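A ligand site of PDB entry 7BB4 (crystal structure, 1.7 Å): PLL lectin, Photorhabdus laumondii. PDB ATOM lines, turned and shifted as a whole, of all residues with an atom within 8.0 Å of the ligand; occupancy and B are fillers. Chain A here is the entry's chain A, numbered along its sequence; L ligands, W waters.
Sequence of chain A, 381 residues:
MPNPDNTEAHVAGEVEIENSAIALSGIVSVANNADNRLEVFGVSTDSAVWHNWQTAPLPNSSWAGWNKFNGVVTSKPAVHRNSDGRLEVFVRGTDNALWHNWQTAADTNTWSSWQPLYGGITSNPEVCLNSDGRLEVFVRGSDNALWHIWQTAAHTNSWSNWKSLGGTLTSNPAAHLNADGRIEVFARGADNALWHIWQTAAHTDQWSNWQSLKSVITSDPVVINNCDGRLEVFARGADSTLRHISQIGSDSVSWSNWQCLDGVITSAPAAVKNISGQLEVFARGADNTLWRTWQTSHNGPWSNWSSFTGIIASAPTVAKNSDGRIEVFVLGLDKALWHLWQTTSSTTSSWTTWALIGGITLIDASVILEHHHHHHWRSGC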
ATOM      1  N   ASN A  96       0.424   7.755  -9.519  1.00  0.00           N
ATOM      2  CA  ASN A  96       0.038   9.081 -10.003  1.00  0.00           C
ATOM      3  C   ASN A  96      -0.564   9.041 -11.401  1.00  0.00           C
ATOM      4  O   ASN A  96      -0.682  10.074 -12.058  1.00  0.00           O
ATOM      5  CB  ASN A  96       1.217  10.060  -9.946  1.00  0.00           C
ATOM      6  CG  ASN A  96       1.489  10.557  -8.548  1.00  0.00           C
ATOM      7  OD1 ASN A  96       0.604  10.543  -7.681  1.00  0.00           O
ATOM      8  ND2 ASN A  96       2.725  10.972  -8.295  1.00  0.00           N
ATOM      9  N   ALA A  97      -0.985   7.868 -11.843  1.00  0.00           N
ATOM     10  CA  ALA A  97      -1.729   7.711 -13.093  1.00  0.00           C
ATOM     11  C   ALA A  97      -3.223   7.642 -12.802  1.00  0.00           C
ATOM     12  O   ALA A  97      -3.650   7.542 -11.655  1.00  0.00           O
ATOM     13  CB  ALA A  97      -1.280   6.436 -13.813  1.00  0.00           C
ATOM     14  N   LEU A  98      -4.006   7.677 -13.866  1.00  0.00           N
ATOM     15  CA  LEU A  98      -5.456   7.597 -13.740  1.00  0.00           C
ATOM     16  C   LEU A  98      -5.908   6.152 -13.786  1.00  0.00           C
ATOM     17  O   LEU A  98      -5.443   5.363 -14.628  1.00  0.00           O
ATOM     18  CB  LEU A  98      -6.132   8.391 -14.870  1.00  0.00           C
ATOM     19  CG  LEU A  98      -7.639   8.494 -14.876  1.00  0.00           C
ATOM     20  CD1 LEU A  98      -8.110   9.301 -13.681  1.00  0.00           C
ATOM     21  CD2 LEU A  98      -8.066   9.160 -16.189  1.00  0.00           C
ATOM     22  N   LEU A 117      -5.692   3.793 -16.880  1.00  0.00           N
ATOM     23  CA  LEU A 117      -5.743   4.703 -18.017  1.00  0.00           C
ATOM     24  C   LEU A 117      -4.446   5.488 -18.175  1.00  0.00           C
ATOM     25  O   LEU A 117      -4.355   6.321 -19.093  1.00  0.00           O
ATOM     26  CB  LEU A 117      -6.955   5.654 -17.868  1.00  0.00           C
ATOM     27  CG  LEU A 117      -8.324   5.003 -18.167  1.00  0.00           C
ATOM     28  CD1 LEU A 117      -9.480   5.912 -17.813  1.00  0.00           C
ATOM     29  CD2 LEU A 117      -8.424   4.529 -19.618  1.00  0.00           C
ATOM     30  N   TYR A 118      -3.448   5.251 -17.322  1.00  0.00           N
ATOM     31  CA  TYR A 118      -2.116   5.824 -17.475  1.00  0.00           C
ATOM     32  C   TYR A 118      -2.145   7.344 -17.315  1.00  0.00           C
ATOM     33  O   TYR A 118      -3.012   7.876 -16.622  1.00  0.00           O
ATOM     34  CB  TYR A 118      -1.511   5.399 -18.816  1.00  0.00           C
ATOM     35  CG  TYR A 118      -1.435   3.887 -18.879  1.00  0.00           C
ATOM     36  CD1 TYR A 118      -0.440   3.207 -18.201  1.00  0.00           C
ATOM     37  CD2 TYR A 118      -2.407   3.146 -19.540  1.00  0.00           C
ATOM     38  CE1 TYR A 118      -0.396   1.829 -18.219  1.00  0.00           C
ATOM     39  CE2 TYR A 118      -2.367   1.756 -19.564  1.00  0.00           C
ATOM     40  CZ  TYR A 118      -1.341   1.109 -18.895  1.00  0.00           C
ATOM     41  OH  TYR A 118      -1.280  -0.267 -18.880  1.00  0.00           O
ATOM     42  N   GLY A 119      -1.174   8.053 -17.891  1.00  0.00           N
ATOM     43  CA  GLY A 119      -1.059   9.483 -17.703  1.00  0.00           C
ATOM     44  C   GLY A 119      -0.327   9.856 -16.421  1.00  0.00           C
ATOM     45  O   GLY A 119      -0.043   9.033 -15.545  1.00  0.00           O
ATOM     46  N   GLY A 120       0.012  11.140 -16.330  1.00  0.00           N
ATOM     47  CA  GLY A 120       0.544  11.738 -15.126  1.00  0.00           C
ATOM     48  C   GLY A 120      -0.411  12.802 -14.644  1.00  0.00           C
ATOM     49  O   GLY A 120      -0.657  13.793 -15.347  1.00  0.00           O
ATOM     50  N   ILE A 121      -0.956  12.622 -13.443  1.00  0.00           N
ATOM     51  CA  ILE A 121      -2.124  13.344 -12.962  1.00  0.00           C
ATOM     52  C   ILE A 121      -1.690  14.219 -11.791  1.00  0.00           C
ATOM     53  O   ILE A 121      -1.082  13.717 -10.848  1.00  0.00           O
ATOM     54  CB  ILE A 121      -3.236  12.374 -12.524  1.00  0.00           C
ATOM     55  CG1 ILE A 121      -3.488  11.311 -13.605  1.00  0.00           C
ATOM     56  CG2 ILE A 121      -4.518  13.109 -12.159  1.00  0.00           C
ATOM     57  CD1 ILE A 121      -3.716  11.873 -14.994  1.00  0.00           C
ATOM     58  N   THR A 122      -2.013  15.516 -11.852  1.00  0.00           N
ATOM     59  CA  THR A 122      -1.674  16.406 -10.750  1.00  0.00           C
ATOM     60  C   THR A 122      -2.911  17.153 -10.229  1.00  0.00           C
ATOM     61  O   THR A 122      -2.759  18.190  -9.582  1.00  0.00           O
ATOM     62  CB  THR A 122      -0.589  17.406 -11.159  1.00  0.00           C
ATOM     63  OG1 THR A 122      -1.110  18.296 -12.155  1.00  0.00           O
ATOM     64  CG2 THR A 122       0.616  16.654 -11.745  1.00  0.00           C
ATOM     65  N   VAL A 139      -8.144  16.405 -16.482  1.00  0.00           N
ATOM     66  CA  VAL A 139      -7.230  16.497 -15.358  1.00  0.00           C
ATOM     67  C   VAL A 139      -6.199  17.583 -15.643  1.00  0.00           C
ATOM     68  O   VAL A 139      -5.940  17.943 -16.782  1.00  0.00           O
ATOM     69  CB  VAL A 139      -6.476  15.174 -15.098  1.00  0.00           C
ATOM     70  CG1 VAL A 139      -7.456  14.010 -14.937  1.00  0.00           C
ATOM     71  CG2 VAL A 139      -5.487  14.908 -16.235  1.00  0.00           C
ATOM     72  N   ARG A 140      -5.588  18.092 -14.563  1.00  0.00           N
ATOM     73  CA  ARG A 140      -4.338  18.808 -14.730  1.00  0.00           C
ATOM     74  C   ARG A 140      -3.227  17.779 -14.874  1.00  0.00           C
ATOM     75  O   ARG A 140      -3.233  16.744 -14.213  1.00  0.00           O
ATOM     76  CB  ARG A 140      -4.047  19.738 -13.550  1.00  0.00           C
ATOM     77  CG  ARG A 140      -2.859  20.663 -13.796  1.00  0.00           C
ATOM     78  CD  ARG A 140      -2.646  21.632 -12.646  1.00  0.00           C
ATOM     79  NE  ARG A 140      -2.154  20.958 -11.452  1.00  0.00           N
ATOM     80  CZ  ARG A 140      -1.786  21.580 -10.329  1.00  0.00           C
ATOM     81  NH1 ARG A 140      -1.857  22.911 -10.245  1.00  0.00           N
ATOM     82  NH2 ARG A 140      -1.344  20.883  -9.298  1.00  0.00           N
ATOM     83  N   GLY A 141      -2.307  18.033 -15.794  1.00  0.00           N
ATOM     84  CA  GLY A 141      -1.252  17.106 -16.113  1.00  0.00           C
ATOM     85  C   GLY A 141       0.076  17.496 -15.467  1.00  0.00           C
ATOM     86  O   GLY A 141       0.171  18.436 -14.680  1.00  0.00           O
ATOM     87  N   SER A 142       1.115  16.739 -15.840  1.00  0.00           N
ATOM     88  CA  SER A 142       2.438  16.917 -15.221  1.00  0.00           C
ATOM     89  C   SER A 142       3.043  18.290 -15.524  1.00  0.00           C
ATOM     90  O   SER A 142       3.918  18.745 -14.785  1.00  0.00           O
ATOM     91  CB  SER A 142       3.392  15.808 -15.681  1.00  0.00           C
ATOM     92  OG  SER A 142       3.543  15.847 -17.098  1.00  0.00           O
ATOM     93  N   ASP A 143       2.602  18.929 -16.607  1.00  0.00           N
ATOM     94  CA  ASP A 143       3.090  20.237 -17.002  1.00  0.00           C
ATOM     95  C   ASP A 143       2.112  21.334 -16.616  1.00  0.00           C
ATOM     96  O   ASP A 143       2.252  22.473 -17.094  1.00  0.00           O
ATOM     97  CB  ASP A 143       3.329  20.263 -18.516  1.00  0.00           C
ATOM     98  CG  ASP A 143       2.072  19.933 -19.306  1.00  0.00           C
ATOM     99  OD1 ASP A 143       1.022  19.628 -18.680  1.00  0.00           O
ATOM    100  OD2 ASP A 143       2.129  19.987 -20.558  1.00  0.00           O
ATOM    101  N   ASN A 144       1.124  21.020 -15.773  1.00  0.00           N
ATOM    102  CA  ASN A 144       0.114  21.923 -15.261  1.00  0.00           C
ATOM    103  C   ASN A 144      -0.896  22.335 -16.316  1.00  0.00           C
ATOM    104  O   ASN A 144      -1.760  23.184 -16.033  1.00  0.00           O
ATOM    105  CB  ASN A 144       0.740  23.172 -14.617  1.00  0.00           C
ATOM    106  CG  ASN A 144       1.474  22.843 -13.335  1.00  0.00           C
ATOM    107  OD1 ASN A 144       0.951  22.108 -12.491  1.00  0.00           O
ATOM    108  ND2 ASN A 144       2.678  23.374 -13.183  1.00  0.00           N
ATOM    109  N   ALA A 145      -0.837  21.754 -17.502  1.00  0.00           N
ATOM    110  CA  ALA A 145      -1.860  22.029 -18.509  1.00  0.00           C
ATOM    111  C   ALA A 145      -3.109  21.166 -18.254  1.00  0.00           C
ATOM    112  O   ALA A 145      -3.106  20.238 -17.441  1.00  0.00           O
ATOM    113  CB  ALA A 145      -1.324  21.778 -19.919  1.00  0.00           C
ATOM    114  N   LEU A 146      -4.188  21.520 -18.953  1.00  0.00           N
ATOM    115  CA  LEU A 146      -5.377  20.675 -19.000  1.00  0.00           C
ATOM    116  C   LEU A 146      -5.185  19.549 -20.002  1.00  0.00           C
ATOM    117  O   LEU A 146      -4.854  19.787 -21.160  1.00  0.00           O
ATOM    118  CB  LEU A 146      -6.606  21.500 -19.388  1.00  0.00           C
ATOM    119  CG  LEU A 146      -7.946  20.743 -19.467  1.00  0.00           C
ATOM    120  CD1 LEU A 146      -8.350  20.223 -18.077  1.00  0.00           C
ATOM    121  CD2 LEU A 146      -9.045  21.643 -20.044  1.00  0.00           C
ATOM    122  N   TRP A 147      -5.418  18.317 -19.565  1.00  0.00           N
ATOM    123  CA  TRP A 147      -5.337  17.149 -20.428  1.00  0.00           C
ATOM    124  C   TRP A 147      -6.660  16.406 -20.365  1.00  0.00           C
ATOM    125  O   TRP A 147      -7.378  16.481 -19.360  1.00  0.00           O
ATOM    126  CB  TRP A 147      -4.203  16.221 -19.992  1.00  0.00           C
ATOM    127  CG  TRP A 147      -2.829  16.767 -20.258  1.00  0.00           C
ATOM    128  CD1 TRP A 147      -2.194  17.759 -19.566  1.00  0.00           C
ATOM    129  CD2 TRP A 147      -1.932  16.364 -21.297  1.00  0.00           C
ATOM    130  NE1 TRP A 147      -0.948  17.985 -20.097  1.00  0.00           N
ATOM    131  CE2 TRP A 147      -0.767  17.149 -21.163  1.00  0.00           C
ATOM    132  CE3 TRP A 147      -2.001  15.401 -22.309  1.00  0.00           C
ATOM    133  CZ2 TRP A 147       0.334  17.005 -22.029  1.00  0.00           C
ATOM    134  CZ3 TRP A 147      -0.896  15.257 -23.162  1.00  0.00           C
ATOM    135  CH2 TRP A 147       0.241  16.063 -23.014  1.00  0.00           C
ATOM    136  N   HIS A 148      -6.993  15.685 -21.439  1.00  0.00           N
ATOM    137  CA  HIS A 148      -8.220  14.906 -21.417  1.00  0.00           C
ATOM    138  C   HIS A 148      -8.063  13.597 -22.197  1.00  0.00           C
ATOM    139  O   HIS A 148      -7.120  13.408 -22.963  1.00  0.00           O
ATOM    140  CB  HIS A 148      -9.425  15.729 -21.921  1.00  0.00           C
ATOM    141  CG  HIS A 148      -9.339  16.224 -23.336  1.00  0.00           C
ATOM    142  ND1 HIS A 148     -10.446  16.302 -24.152  1.00  0.00           N
ATOM    143  CD2 HIS A 148      -8.307  16.713 -24.060  1.00  0.00           C
ATOM    144  CE1 HIS A 148     -10.096  16.792 -25.322  1.00  0.00           C
ATOM    145  NE2 HIS A 148      -8.801  17.049 -25.304  1.00  0.00           N
ATOM    146  N   ILE A 149      -8.993  12.687 -21.925  1.00  0.00           N
ATOM    147  CA  ILE A 149      -9.017  11.346 -22.496  1.00  0.00           C
ATOM    148  C   ILE A 149     -10.485  10.944 -22.519  1.00  0.00           C
ATOM    149  O   ILE A 149     -11.272  11.406 -21.686  1.00  0.00           O
ATOM    150  CB  ILE A 149      -8.145  10.384 -21.660  1.00  0.00           C
ATOM    151  CG1 ILE A 149      -7.938   9.057 -22.395  1.00  0.00           C
ATOM    152  CG2 ILE A 149      -8.727  10.194 -20.259  1.00  0.00           C
ATOM    153  CD1 ILE A 149      -7.025   8.065 -21.651  1.00  0.00           C
ATOM    154  N   TRP A 162      -4.180  10.137 -24.415  1.00  0.00           N
ATOM    155  CA  TRP A 162      -4.171  11.429 -23.737  1.00  0.00           C
ATOM    156  C   TRP A 162      -3.853  12.551 -24.709  1.00  0.00           C
ATOM    157  O   TRP A 162      -3.000  12.415 -25.590  1.00  0.00           O
ATOM    158  CB  TRP A 162      -3.134  11.416 -22.625  1.00  0.00           C
ATOM    159  CG  TRP A 162      -3.577  10.705 -21.392  1.00  0.00           C
ATOM    160  CD1 TRP A 162      -3.226   9.419 -21.009  1.00  0.00           C
ATOM    161  CD2 TRP A 162      -4.462  11.191 -20.394  1.00  0.00           C
ATOM    162  NE1 TRP A 162      -3.827   9.114 -19.816  1.00  0.00           N
ATOM    163  CE2 TRP A 162      -4.586  10.180 -19.415  1.00  0.00           C
ATOM    164  CE3 TRP A 162      -5.145  12.401 -20.204  1.00  0.00           C
ATOM    165  CZ2 TRP A 162      -5.379  10.344 -18.273  1.00  0.00           C
ATOM    166  CZ3 TRP A 162      -5.925  12.560 -19.080  1.00  0.00           C
ATOM    167  CH2 TRP A 162      -6.042  11.533 -18.125  1.00  0.00           C
ATOM    168  N   LYS A 163      -4.529  13.690 -24.536  1.00  0.00           N
ATOM    169  CA  LYS A 163      -4.319  14.838 -25.406  1.00  0.00           C
ATOM    170  C   LYS A 163      -4.357  16.111 -24.585  1.00  0.00           C
ATOM    171  O   LYS A 163      -5.121  16.216 -23.618  1.00  0.00           O
ATOM    172  CB  LYS A 163      -5.373  14.898 -26.515  1.00  0.00           C
ATOM    173  CG  LYS A 163      -5.102  15.967 -27.562  1.00  0.00           C
ATOM    174  CD  LYS A 163      -5.928  15.708 -28.826  1.00  0.00           C
ATOM    175  CE  LYS A 163      -5.670  16.763 -29.885  1.00  0.00           C
ATOM    176  NZ  LYS A 163      -6.393  16.411 -31.133  1.00  0.00           N
ATOM    177  N   SER A 164      -3.540  17.088 -24.980  1.00  0.00           N
ATOM    178  CA  SER A 164      -3.398  18.300 -24.185  1.00  0.00           C
ATOM    179  C   SER A 164      -4.305  19.402 -24.718  1.00  0.00           C
ATOM    180  O   SER A 164      -4.431  19.590 -25.937  1.00  0.00           O
ATOM    181  CB  SER A 164      -1.959  18.801 -24.183  1.00  0.00           C
ATOM    182  OG  SER A 164      -1.872  20.062 -23.556  1.00  0.00           O
HETATM  183  C1  LIG L   1       0.950  12.114 -20.053  1.00  0.00           C
HETATM  184  C2  LIG L   1       1.954  13.234 -19.781  1.00  0.00           C
HETATM  185  O1  LIG L   1       2.990  13.186 -20.784  1.00  0.00           O
HETATM  186  C3  LIG L   1       1.259  14.547 -19.837  1.00  0.00           C
HETATM  187  O2  LIG L   1       2.227  15.598 -19.534  1.00  0.00           O
HETATM  188  C4  LIG L   1       0.092  14.639 -18.880  1.00  0.00           C
HETATM  189  O3  LIG L   1       0.599  14.597 -17.545  1.00  0.00           O
HETATM  190  C5  LIG L   1      -0.915  13.502 -19.100  1.00  0.00           C
HETATM  191  C6  LIG L   1      -1.970  13.538 -18.041  1.00  0.00           C
HETATM  192  O4  LIG L   1      -0.217  12.196 -19.110  1.00  0.00           O
HETATM  193  O5  LIG L   1       1.505  10.878 -19.886  1.00  0.00           O
HETATM  194  O   HOH W   1       3.258  10.111 -18.254  1.00  0.00           O
HETATM  195  O   HOH W   2       3.972  16.029 -21.694  1.00  0.00           O
HETATM  196  O   HOH W   3       2.061  12.549 -23.287  1.00  0.00           O
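Merely in contact with the ligand: Gly 119 (3.2 Å), Trp 147 (3.4 Å), Gly 141 (3.4 Å) and Ile 121 (3.9 Å). Within 4 Å of the ligand: Gly 119, Gly 120, Ile 121, Gly 141, Ser 142 and Trp 147.
An oxygen (O4) of the ligand sits at hydrogen-bond distance from the backbone NH (N) of Gly 120 (3.0 Å). The backbone carbonyl oxygen (O) of Gly 120 is in hydrogen-bond range of an oxygen (O3) of the ligand (2.7 Å). N of Ser 142 sits at hydrogen-bond distance from O3 of the ligand (2.8 Å). An oxygen (O2) of the ligand is in hydrogen-bond range of the side-chain hydroxyl (OG) of Ser 142 (2.8 Å).
O of Gly 120 is in hydrogen-bond range of N of Ser 142, at 3.5 Å. The backbone NH of Trp 147 sits at hydrogen-bond distance from the backbone carbonyl oxygen of Val 139 (2.9 Å). NE1 of Trp 147 is in hydrogen-bond range of OD1 of Asp 143 (2.9 Å). O of Gly 141 is in hydrogen-bond range of OG1 of Thr 122 (2.8 Å). The backbone carbonyl oxygen (O) of Asn 96 lies within hydrogen-bond range of the backbone NH (N) of Ile 121, at 2.9 Å.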
